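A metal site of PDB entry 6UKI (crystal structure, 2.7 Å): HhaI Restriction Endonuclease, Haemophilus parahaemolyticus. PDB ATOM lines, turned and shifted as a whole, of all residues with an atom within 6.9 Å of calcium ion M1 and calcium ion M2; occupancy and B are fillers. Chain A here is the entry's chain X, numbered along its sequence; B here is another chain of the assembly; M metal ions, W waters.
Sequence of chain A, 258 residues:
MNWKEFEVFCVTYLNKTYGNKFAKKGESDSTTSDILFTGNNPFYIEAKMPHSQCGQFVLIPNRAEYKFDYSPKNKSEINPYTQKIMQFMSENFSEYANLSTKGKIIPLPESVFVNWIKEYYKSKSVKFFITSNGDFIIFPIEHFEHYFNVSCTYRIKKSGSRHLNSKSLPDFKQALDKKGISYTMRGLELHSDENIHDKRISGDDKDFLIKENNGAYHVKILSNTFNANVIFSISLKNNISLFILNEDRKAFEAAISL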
ATOM      1  N   TRP A   3      -6.968 -13.152  17.701  1.00  0.00           N
ATOM      2  CA  TRP A   3      -8.145 -13.735  17.066  1.00  0.00           C
ATOM      3  C   TRP A   3      -7.800 -14.459  15.783  1.00  0.00           C
ATOM      4  O   TRP A   3      -8.478 -15.423  15.414  1.00  0.00           O
ATOM      5  CB  TRP A   3      -9.200 -12.662  16.790  1.00  0.00           C
ATOM      6  CG  TRP A   3      -8.780 -11.628  15.789  1.00  0.00           C
ATOM      7  CD1 TRP A   3      -8.212 -10.416  16.057  1.00  0.00           C
ATOM      8  CD2 TRP A   3      -8.890 -11.704  14.356  1.00  0.00           C
ATOM      9  NE1 TRP A   3      -7.974  -9.731  14.888  1.00  0.00           N
ATOM     10  CE2 TRP A   3      -8.381 -10.508  13.829  1.00  0.00           C
ATOM     11  CE3 TRP A   3      -9.371 -12.678  13.477  1.00  0.00           C
ATOM     12  CZ2 TRP A   3      -8.332 -10.253  12.463  1.00  0.00           C
ATOM     13  CZ3 TRP A   3      -9.332 -12.419  12.113  1.00  0.00           C
ATOM     14  CH2 TRP A   3      -8.813 -11.217  11.625  1.00  0.00           C
ATOM     15  N   GLU A   7      -8.963 -18.477  14.977  1.00  0.00           N
ATOM     16  CA  GLU A   7      -9.633 -19.060  13.818  1.00  0.00           C
ATOM     17  C   GLU A   7      -8.863 -20.270  13.293  1.00  0.00           C
ATOM     18  O   GLU A   7      -9.467 -21.299  12.948  1.00  0.00           O
ATOM     19  CB  GLU A   7      -9.786 -18.016  12.703  1.00  0.00           C
ATOM     20  CG  GLU A   7     -11.139 -17.338  12.611  1.00  0.00           C
ATOM     21  CD  GLU A   7     -11.219 -16.365  11.450  1.00  0.00           C
ATOM     22  OE1 GLU A   7     -11.922 -15.334  11.563  1.00  0.00           O
ATOM     23  OE2 GLU A   7     -10.566 -16.625  10.404  1.00  0.00           O
ATOM     24  N   LYS A  25     -11.694 -19.162   5.076  1.00  0.00           N
ATOM     25  CA  LYS A  25     -11.710 -17.975   4.235  1.00  0.00           C
ATOM     26  C   LYS A  25     -10.760 -16.911   4.806  1.00  0.00           C
ATOM     27  O   LYS A  25     -10.063 -17.123   5.795  1.00  0.00           O
ATOM     28  CB  LYS A  25     -13.133 -17.450   4.104  1.00  0.00           C
ATOM     29  CG  LYS A  25     -14.090 -18.454   3.479  1.00  0.00           C
ATOM     30  CD  LYS A  25     -14.025 -18.392   1.959  1.00  0.00           C
ATOM     31  CE  LYS A  25     -15.332 -18.846   1.344  1.00  0.00           C
ATOM     32  NZ  LYS A  25     -16.292 -17.722   1.183  1.00  0.00           N
ATOM     33  N   GLY A  26     -10.747 -15.736   4.172  1.00  0.00           N
ATOM     34  CA  GLY A  26      -9.848 -14.685   4.596  1.00  0.00           C
ATOM     35  C   GLY A  26     -10.175 -14.171   5.986  1.00  0.00           C
ATOM     36  O   GLY A  26     -11.335 -14.115   6.391  1.00  0.00           O
ATOM     37  N   GLU A  27      -9.126 -13.799   6.714  1.00  0.00           N
ATOM     38  CA  GLU A  27      -9.248 -13.339   8.094  1.00  0.00           C
ATOM     39  C   GLU A  27     -10.175 -12.136   8.212  1.00  0.00           C
ATOM     40  O   GLU A  27     -11.252 -12.226   8.824  1.00  0.00           O
ATOM     41  CB  GLU A  27      -7.873 -12.966   8.662  1.00  0.00           C
ATOM     42  CG  GLU A  27      -6.773 -13.996   8.432  1.00  0.00           C
ATOM     43  CD  GLU A  27      -5.419 -13.512   8.924  1.00  0.00           C
ATOM     44  OE1 GLU A  27      -4.530 -14.360   9.153  1.00  0.00           O
ATOM     45  OE2 GLU A  27      -5.245 -12.290   9.097  1.00  0.00           O
ATOM     46  N   SER A  28      -9.762 -11.015   7.616  1.00  0.00           N
ATOM     47  CA  SER A  28     -10.494  -9.751   7.697  1.00  0.00           C
ATOM     48  C   SER A  28     -11.382  -9.521   6.490  1.00  0.00           C
ATOM     49  O   SER A  28     -11.645  -8.376   6.128  1.00  0.00           O
ATOM     50  CB  SER A  28      -9.513  -8.589   7.870  1.00  0.00           C
ATOM     51  OG  SER A  28      -8.443  -8.931   8.731  1.00  0.00           O
ATOM     52  N   ASP A  29     -11.855 -10.599   5.861  1.00  0.00           N
ATOM     53  CA  ASP A  29     -12.697 -10.553   4.668  1.00  0.00           C
ATOM     54  C   ASP A  29     -14.142 -10.290   5.078  1.00  0.00           C
ATOM     55  O   ASP A  29     -14.796 -11.166   5.647  1.00  0.00           O
ATOM     56  CB  ASP A  29     -12.564 -11.859   3.904  1.00  0.00           C
ATOM     57  CG  ASP A  29     -13.183 -11.809   2.523  1.00  0.00           C
ATOM     58  OD1 ASP A  29     -14.283 -11.235   2.370  1.00  0.00           O
ATOM     59  OD2 ASP A  29     -12.555 -12.358   1.590  1.00  0.00           O
ATOM     60  N   SER A  30     -14.642  -9.101   4.759  1.00  0.00           N
ATOM     61  CA  SER A  30     -15.963  -8.698   5.231  1.00  0.00           C
ATOM     62  C   SER A  30     -17.105  -9.435   4.536  1.00  0.00           C
ATOM     63  O   SER A  30     -18.233  -9.420   5.034  1.00  0.00           O
ATOM     64  CB  SER A  30     -16.110  -7.190   5.057  1.00  0.00           C
ATOM     65  OG  SER A  30     -17.442  -6.823   4.747  1.00  0.00           O
ATOM     66  N   THR A  32     -17.870 -12.712   3.612  1.00  0.00           N
ATOM     67  CA  THR A  32     -18.361 -14.053   3.878  1.00  0.00           C
ATOM     68  C   THR A  32     -18.081 -14.420   5.335  1.00  0.00           C
ATOM     69  O   THR A  32     -17.396 -13.688   6.063  1.00  0.00           O
ATOM     70  CB  THR A  32     -17.710 -15.068   2.933  1.00  0.00           C
ATOM     71  OG1 THR A  32     -18.469 -16.278   2.901  1.00  0.00           O
ATOM     72  CG2 THR A  32     -16.286 -15.373   3.381  1.00  0.00           C
ATOM     73  N   SER A  33     -18.619 -15.566   5.760  1.00  0.00           N
ATOM     74  CA  SER A  33     -18.355 -16.104   7.078  1.00  0.00           C
ATOM     75  C   SER A  33     -17.056 -16.927   7.070  1.00  0.00           C
ATOM     76  O   SER A  33     -16.434 -17.129   6.023  1.00  0.00           O
ATOM     77  CB  SER A  33     -19.542 -16.933   7.553  1.00  0.00           C
ATOM     78  OG  SER A  33     -19.469 -17.144   8.949  1.00  0.00           O
ATOM     79  N   ASP A  34     -16.666 -17.444   8.234  1.00  0.00           N
ATOM     80  CA  ASP A  34     -15.279 -17.840   8.484  1.00  0.00           C
ATOM     81  C   ASP A  34     -14.902 -19.146   7.803  1.00  0.00           C
ATOM     82  O   ASP A  34     -13.882 -19.212   7.109  1.00  0.00           O
ATOM     83  CB  ASP A  34     -15.033 -17.968   9.991  1.00  0.00           C
ATOM     84  CG  ASP A  34     -15.141 -16.637  10.715  1.00  0.00           C
ATOM     85  OD1 ASP A  34     -15.124 -15.593  10.036  1.00  0.00           O
ATOM     86  OD2 ASP A  34     -15.239 -16.647  11.961  1.00  0.00           O
ATOM     87  N   ILE A  45     -19.619 -22.135   9.053  1.00  0.00           N
ATOM     88  CA  ILE A  45     -19.390 -22.196  10.488  1.00  0.00           C
ATOM     89  C   ILE A  45     -18.700 -20.903  10.892  1.00  0.00           C
ATOM     90  O   ILE A  45     -17.686 -20.527  10.308  1.00  0.00           O
ATOM     91  CB  ILE A  45     -18.512 -23.397  10.873  1.00  0.00           C
ATOM     92  CG1 ILE A  45     -19.127 -24.706  10.368  1.00  0.00           C
ATOM     93  CG2 ILE A  45     -18.290 -23.449  12.381  1.00  0.00           C
ATOM     94  CD1 ILE A  45     -18.173 -25.878  10.473  1.00  0.00           C
ATOM     95  N   GLU A  46     -19.252 -20.227  11.901  1.00  0.00           N
ATOM     96  CA  GLU A  46     -18.714 -18.948  12.351  1.00  0.00           C
ATOM     97  C   GLU A  46     -17.897 -19.141  13.632  1.00  0.00           C
ATOM     98  O   GLU A  46     -18.428 -19.649  14.631  1.00  0.00           O
ATOM     99  CB  GLU A  46     -19.839 -17.950  12.581  1.00  0.00           C
ATOM    100  CG  GLU A  46     -19.378 -16.574  13.051  1.00  0.00           C
ATOM    101  CD  GLU A  46     -18.537 -15.838  12.029  1.00  0.00           C
ATOM    102  OE1 GLU A  46     -17.950 -14.803  12.397  1.00  0.00           O
ATOM    103  OE2 GLU A  46     -18.462 -16.280  10.859  1.00  0.00           O
ATOM    104  N   ALA A  47     -16.636 -18.728  13.600  1.00  0.00           N
ATOM    105  CA  ALA A  47     -15.753 -18.770  14.768  1.00  0.00           C
ATOM    106  C   ALA A  47     -15.791 -17.436  15.504  1.00  0.00           C
ATOM    107  O   ALA A  47     -15.715 -16.377  14.881  1.00  0.00           O
ATOM    108  CB  ALA A  47     -14.318 -19.070  14.325  1.00  0.00           C
ATOM    109  N   LYS A  48     -15.914 -17.484  16.830  1.00  0.00           N
ATOM    110  CA  LYS A  48     -15.903 -16.274  17.649  1.00  0.00           C
ATOM    111  C   LYS A  48     -15.228 -16.563  18.976  1.00  0.00           C
ATOM    112  O   LYS A  48     -15.487 -17.609  19.582  1.00  0.00           O
ATOM    113  CB  LYS A  48     -17.329 -15.750  17.913  1.00  0.00           C
ATOM    114  CG  LYS A  48     -18.044 -15.296  16.658  1.00  0.00           C
ATOM    115  CD  LYS A  48     -19.069 -14.236  16.944  1.00  0.00           C
ATOM    116  CE  LYS A  48     -19.173 -13.305  15.740  1.00  0.00           C
ATOM    117  NZ  LYS A  48     -17.806 -12.995  15.209  1.00  0.00           N
ATOM    118  N   MET A  49     -14.373 -15.658  19.430  1.00  0.00           N
ATOM    119  CA  MET A  49     -13.725 -15.813  20.724  1.00  0.00           C
ATOM    120  C   MET A  49     -14.737 -15.634  21.855  1.00  0.00           C
ATOM    121  O   MET A  49     -15.843 -15.131  21.644  1.00  0.00           O
ATOM    122  CB  MET A  49     -12.561 -14.836  20.876  1.00  0.00           C
ATOM    123  CG  MET A  49     -11.226 -15.364  20.400  1.00  0.00           C
ATOM    124  SD  MET A  49     -10.024 -14.077  19.994  1.00  0.00           S
ATOM    125  CE  MET A  49      -8.843 -14.254  21.315  1.00  0.00           C
ATOM    126  N   GLN A  53     -17.244  -9.125  19.167  1.00  0.00           N
ATOM    127  CA  GLN A  53     -18.352  -8.360  18.610  1.00  0.00           C
ATOM    128  C   GLN A  53     -19.036  -9.193  17.537  1.00  0.00           C
ATOM    129  O   GLN A  53     -18.516 -10.214  17.082  1.00  0.00           O
ATOM    130  CB  GLN A  53     -17.850  -7.019  18.069  1.00  0.00           C
ATOM    131  CG  GLN A  53     -17.307  -6.152  19.203  1.00  0.00           C
ATOM    132  CD  GLN A  53     -16.501  -4.976  18.730  1.00  0.00           C
ATOM    133  OE1 GLN A  53     -16.920  -3.827  18.873  1.00  0.00           O
ATOM    134  NE2 GLN A  53     -15.320  -5.238  18.179  1.00  0.00           N
ATOM    135  N   TYR A 121     -26.924 -13.799  10.720  1.00  0.00           N
ATOM    136  CA  TYR A 121     -26.017 -14.870  10.346  1.00  0.00           C
ATOM    137  C   TYR A 121     -26.711 -15.952   9.510  1.00  0.00           C
ATOM    138  O   TYR A 121     -26.062 -16.557   8.650  1.00  0.00           O
ATOM    139  CB  TYR A 121     -25.368 -15.459  11.604  1.00  0.00           C
ATOM    140  CG  TYR A 121     -24.198 -14.611  12.055  1.00  0.00           C
ATOM    141  CD1 TYR A 121     -23.001 -14.609  11.328  1.00  0.00           C
ATOM    142  CD2 TYR A 121     -24.294 -13.764  13.151  1.00  0.00           C
ATOM    143  CE1 TYR A 121     -21.940 -13.808  11.706  1.00  0.00           C
ATOM    144  CE2 TYR A 121     -23.240 -12.961  13.540  1.00  0.00           C
ATOM    145  CZ  TYR A 121     -22.055 -12.987  12.811  1.00  0.00           C
ATOM    146  OH  TYR A 121     -20.998 -12.196  13.188  1.00  0.00           O
ATOM    147  P    DG B   8     -19.454  -8.393   9.531  1.00  0.00           P
ATOM    148  OP1  DG B   8     -19.967  -9.758   9.251  1.00  0.00           O
ATOM    149  OP2  DG B   8     -19.930  -7.629  10.712  1.00  0.00           O
ATOM    150  O5'  DG B   8     -17.874  -8.546   9.603  1.00  0.00           O
ATOM    151  C5'  DG B   8     -17.230  -9.489   8.767  1.00  0.00           C
ATOM    152  C4'  DG B   8     -15.772  -9.575   9.134  1.00  0.00           C
ATOM    153  O4'  DG B   8     -15.178  -8.290   8.900  1.00  0.00           O
ATOM    154  C3'  DG B   8     -15.499  -9.885  10.598  1.00  0.00           C
ATOM    155  O3'  DG B   8     -15.366 -11.302  10.793  1.00  0.00           O
ATOM    156  C2'  DG B   8     -14.190  -9.162  10.877  1.00  0.00           C
ATOM    157  C1'  DG B   8     -14.185  -8.017   9.866  1.00  0.00           C
ATOM    158  N9   DG B   8     -14.449  -6.708  10.424  1.00  0.00           N
ATOM    159  C8   DG B   8     -15.673  -6.112  10.601  1.00  0.00           C
ATOM    160  N7   DG B   8     -15.597  -4.912  11.107  1.00  0.00           N
ATOM    161  C5   DG B   8     -14.234  -4.694  11.255  1.00  0.00           C
ATOM    162  C6   DG B   8     -13.547  -3.567  11.732  1.00  0.00           C
ATOM    163  O6   DG B   8     -14.026  -2.506  12.136  1.00  0.00           O
ATOM    164  N1   DG B   8     -12.173  -3.758  11.713  1.00  0.00           N
ATOM    165  C2   DG B   8     -11.546  -4.902  11.283  1.00  0.00           C
ATOM    166  N2   DG B   8     -10.200  -4.900  11.338  1.00  0.00           N
ATOM    167  N3   DG B   8     -12.182  -5.965  10.827  1.00  0.00           N
ATOM    168  C4   DG B   8     -13.519  -5.790  10.840  1.00  0.00           C
ATOM    169  P    DC B   9     -15.492 -11.965  12.255  1.00  0.00           P
ATOM    170  OP1  DC B   9     -15.030 -13.350  12.101  1.00  0.00           O
ATOM    171  OP2  DC B   9     -16.799 -11.652  12.847  1.00  0.00           O
ATOM    172  O5'  DC B   9     -14.382 -11.215  13.128  1.00  0.00           O
ATOM    173  C5'  DC B   9     -13.053 -11.610  13.021  1.00  0.00           C
ATOM    174  C4'  DC B   9     -12.138 -10.684  13.794  1.00  0.00           C
ATOM    175  O4'  DC B   9     -12.143  -9.364  13.218  1.00  0.00           O
ATOM    176  C3'  DC B   9     -12.532 -10.427  15.234  1.00  0.00           C
ATOM    177  O3'  DC B   9     -12.222 -11.552  16.038  1.00  0.00           O
ATOM    178  C2'  DC B   9     -11.616  -9.234  15.530  1.00  0.00           C
ATOM    179  C1'  DC B   9     -11.767  -8.430  14.227  1.00  0.00           C
ATOM    180  N1   DC B   9     -12.808  -7.362  14.323  1.00  0.00           N
ATOM    181  C2   DC B   9     -12.467  -6.100  14.815  1.00  0.00           C
ATOM    182  O2   DC B   9     -11.299  -5.885  15.127  1.00  0.00           O
ATOM    183  N3   DC B   9     -13.428  -5.153  14.908  1.00  0.00           N
ATOM    184  C4   DC B   9     -14.683  -5.426  14.550  1.00  0.00           C
ATOM    185  N4   DC B   9     -15.598  -4.456  14.661  1.00  0.00           N
ATOM    186  C5   DC B   9     -15.063  -6.705  14.061  1.00  0.00           C
ATOM    187  C6   DC B   9     -14.108  -7.638  13.969  1.00  0.00           C
ATOM    188  P    DT B  10     -13.324 -12.186  17.010  1.00  0.00           P
ATOM    189  OP1  DT B  10     -12.776 -13.459  17.507  1.00  0.00           O
ATOM    190  OP2  DT B  10     -14.638 -12.153  16.317  1.00  0.00           O
ATOM    191  O5'  DT B  10     -13.412 -11.165  18.245  1.00  0.00           O
ATOM    192  C5'  DT B  10     -12.425 -11.187  19.261  1.00  0.00           C
ATOM    193  C4'  DT B  10     -11.408 -10.084  19.059  1.00  0.00           C
ATOM    194  O4'  DT B  10     -12.069  -8.782  19.075  1.00  0.00           O
ATOM    195  C3'  DT B  10     -10.300 -10.018  20.121  1.00  0.00           C
ATOM    196  O3'  DT B  10      -9.064  -9.723  19.492  1.00  0.00           O
ATOM    197  C2'  DT B  10     -10.762  -8.874  21.029  1.00  0.00           C
ATOM    198  C1'  DT B  10     -11.430  -7.935  20.044  1.00  0.00           C
ATOM    199  N1   DT B  10     -12.485  -7.022  20.651  1.00  0.00           N
ATOM    200  C2   DT B  10     -12.446  -5.662  20.379  1.00  0.00           C
ATOM    201  O2   DT B  10     -11.592  -5.137  19.708  1.00  0.00           O
ATOM    202  N3   DT B  10     -13.465  -4.937  20.951  1.00  0.00           N
ATOM    203  C4   DT B  10     -14.490  -5.419  21.738  1.00  0.00           C
ATOM    204  O4   DT B  10     -15.344  -4.681  22.211  1.00  0.00           O
ATOM    205  C5   DT B  10     -14.473  -6.843  21.977  1.00  0.00           C
ATOM    206  C7   DT B  10     -15.539  -7.474  22.823  1.00  0.00           C
ATOM    207  C6   DT B  10     -13.484  -7.568  21.428  1.00  0.00           C
HETATM  208 CA    CA M   1     -15.841 -14.891  13.275  1.00  0.00          CA
HETATM  209 CA    CA M   2     -14.628 -13.450   9.431  1.00  0.00          CA
HETATM  210  O   HOH W   1     -16.983 -13.709   9.547  1.00  0.00           O
HETATM  211  O   HOH W   2     -13.743 -15.569  13.361  1.00  0.00           O
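OP2 of DC 9 of chain B lies within salt-bridge range of the side-chain amino group (NZ) of Lys 48 (2.9 Å). O of Asp 34 sits at hydrogen-bond distance from N of Lys 25 (3.0 Å). NZ of Lys 48 sits close to OE1 of Glu 46, at 3.3 Å. The side-chain amino group (NZ) of Lys 48 is in salt-bridge range of OP2 of DT 10 of chain B, at 3.5 Å. The side-chain amino group (NZ) of Lys 48 is in hydrogen-bond range of the backbone carbonyl oxygen (O) of Gln 53 (3.4 Å).
Lys 48 touches calcium ion M1. Within 4 Å of calcium ion M1: Asp 34, Glu 46, Ala 47, Lys 48 and DC 9 of chain B. The nearest printed residue that does not touch calcium ion M1 is DT 10 of chain B (4.3 Å).
Glu 7 touches calcium ion M2. O of Glu 27 touches calcium ion M2, at 3.6 Å. Within 4 Å of calcium ion M2: Glu 7, Glu 27, Asp 34, DG 8 of chain B and DC 9 of chain B. The nearest printed residue that does not touch calcium ion M2 is Thr 32 (4.4 Å).
Calcium ion M1 is bound by OP1 of DC 9 of chain B, 2.1 Å away. The backbone carbonyl oxygen (O) of Ala 47 is bound to calcium ion M1, at 2.2 Å. Water W2 binds calcium ion M1, 2.2 Å away. OD2 of Asp 34 is bound to calcium ion M1, at 2.3 Å. Calcium ion M1 is bound by the side-chain carboxylate (OE1) of Glu 46, 2.3 Å away.
Calcium ion M2 is bound by OD1 of Asp 34 (2.3 Å), water W1 (2.4 Å), O3' of DG 8 of chain B (2.6 Å) and OP1 of DC 9 of chain B (2.7 Å).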
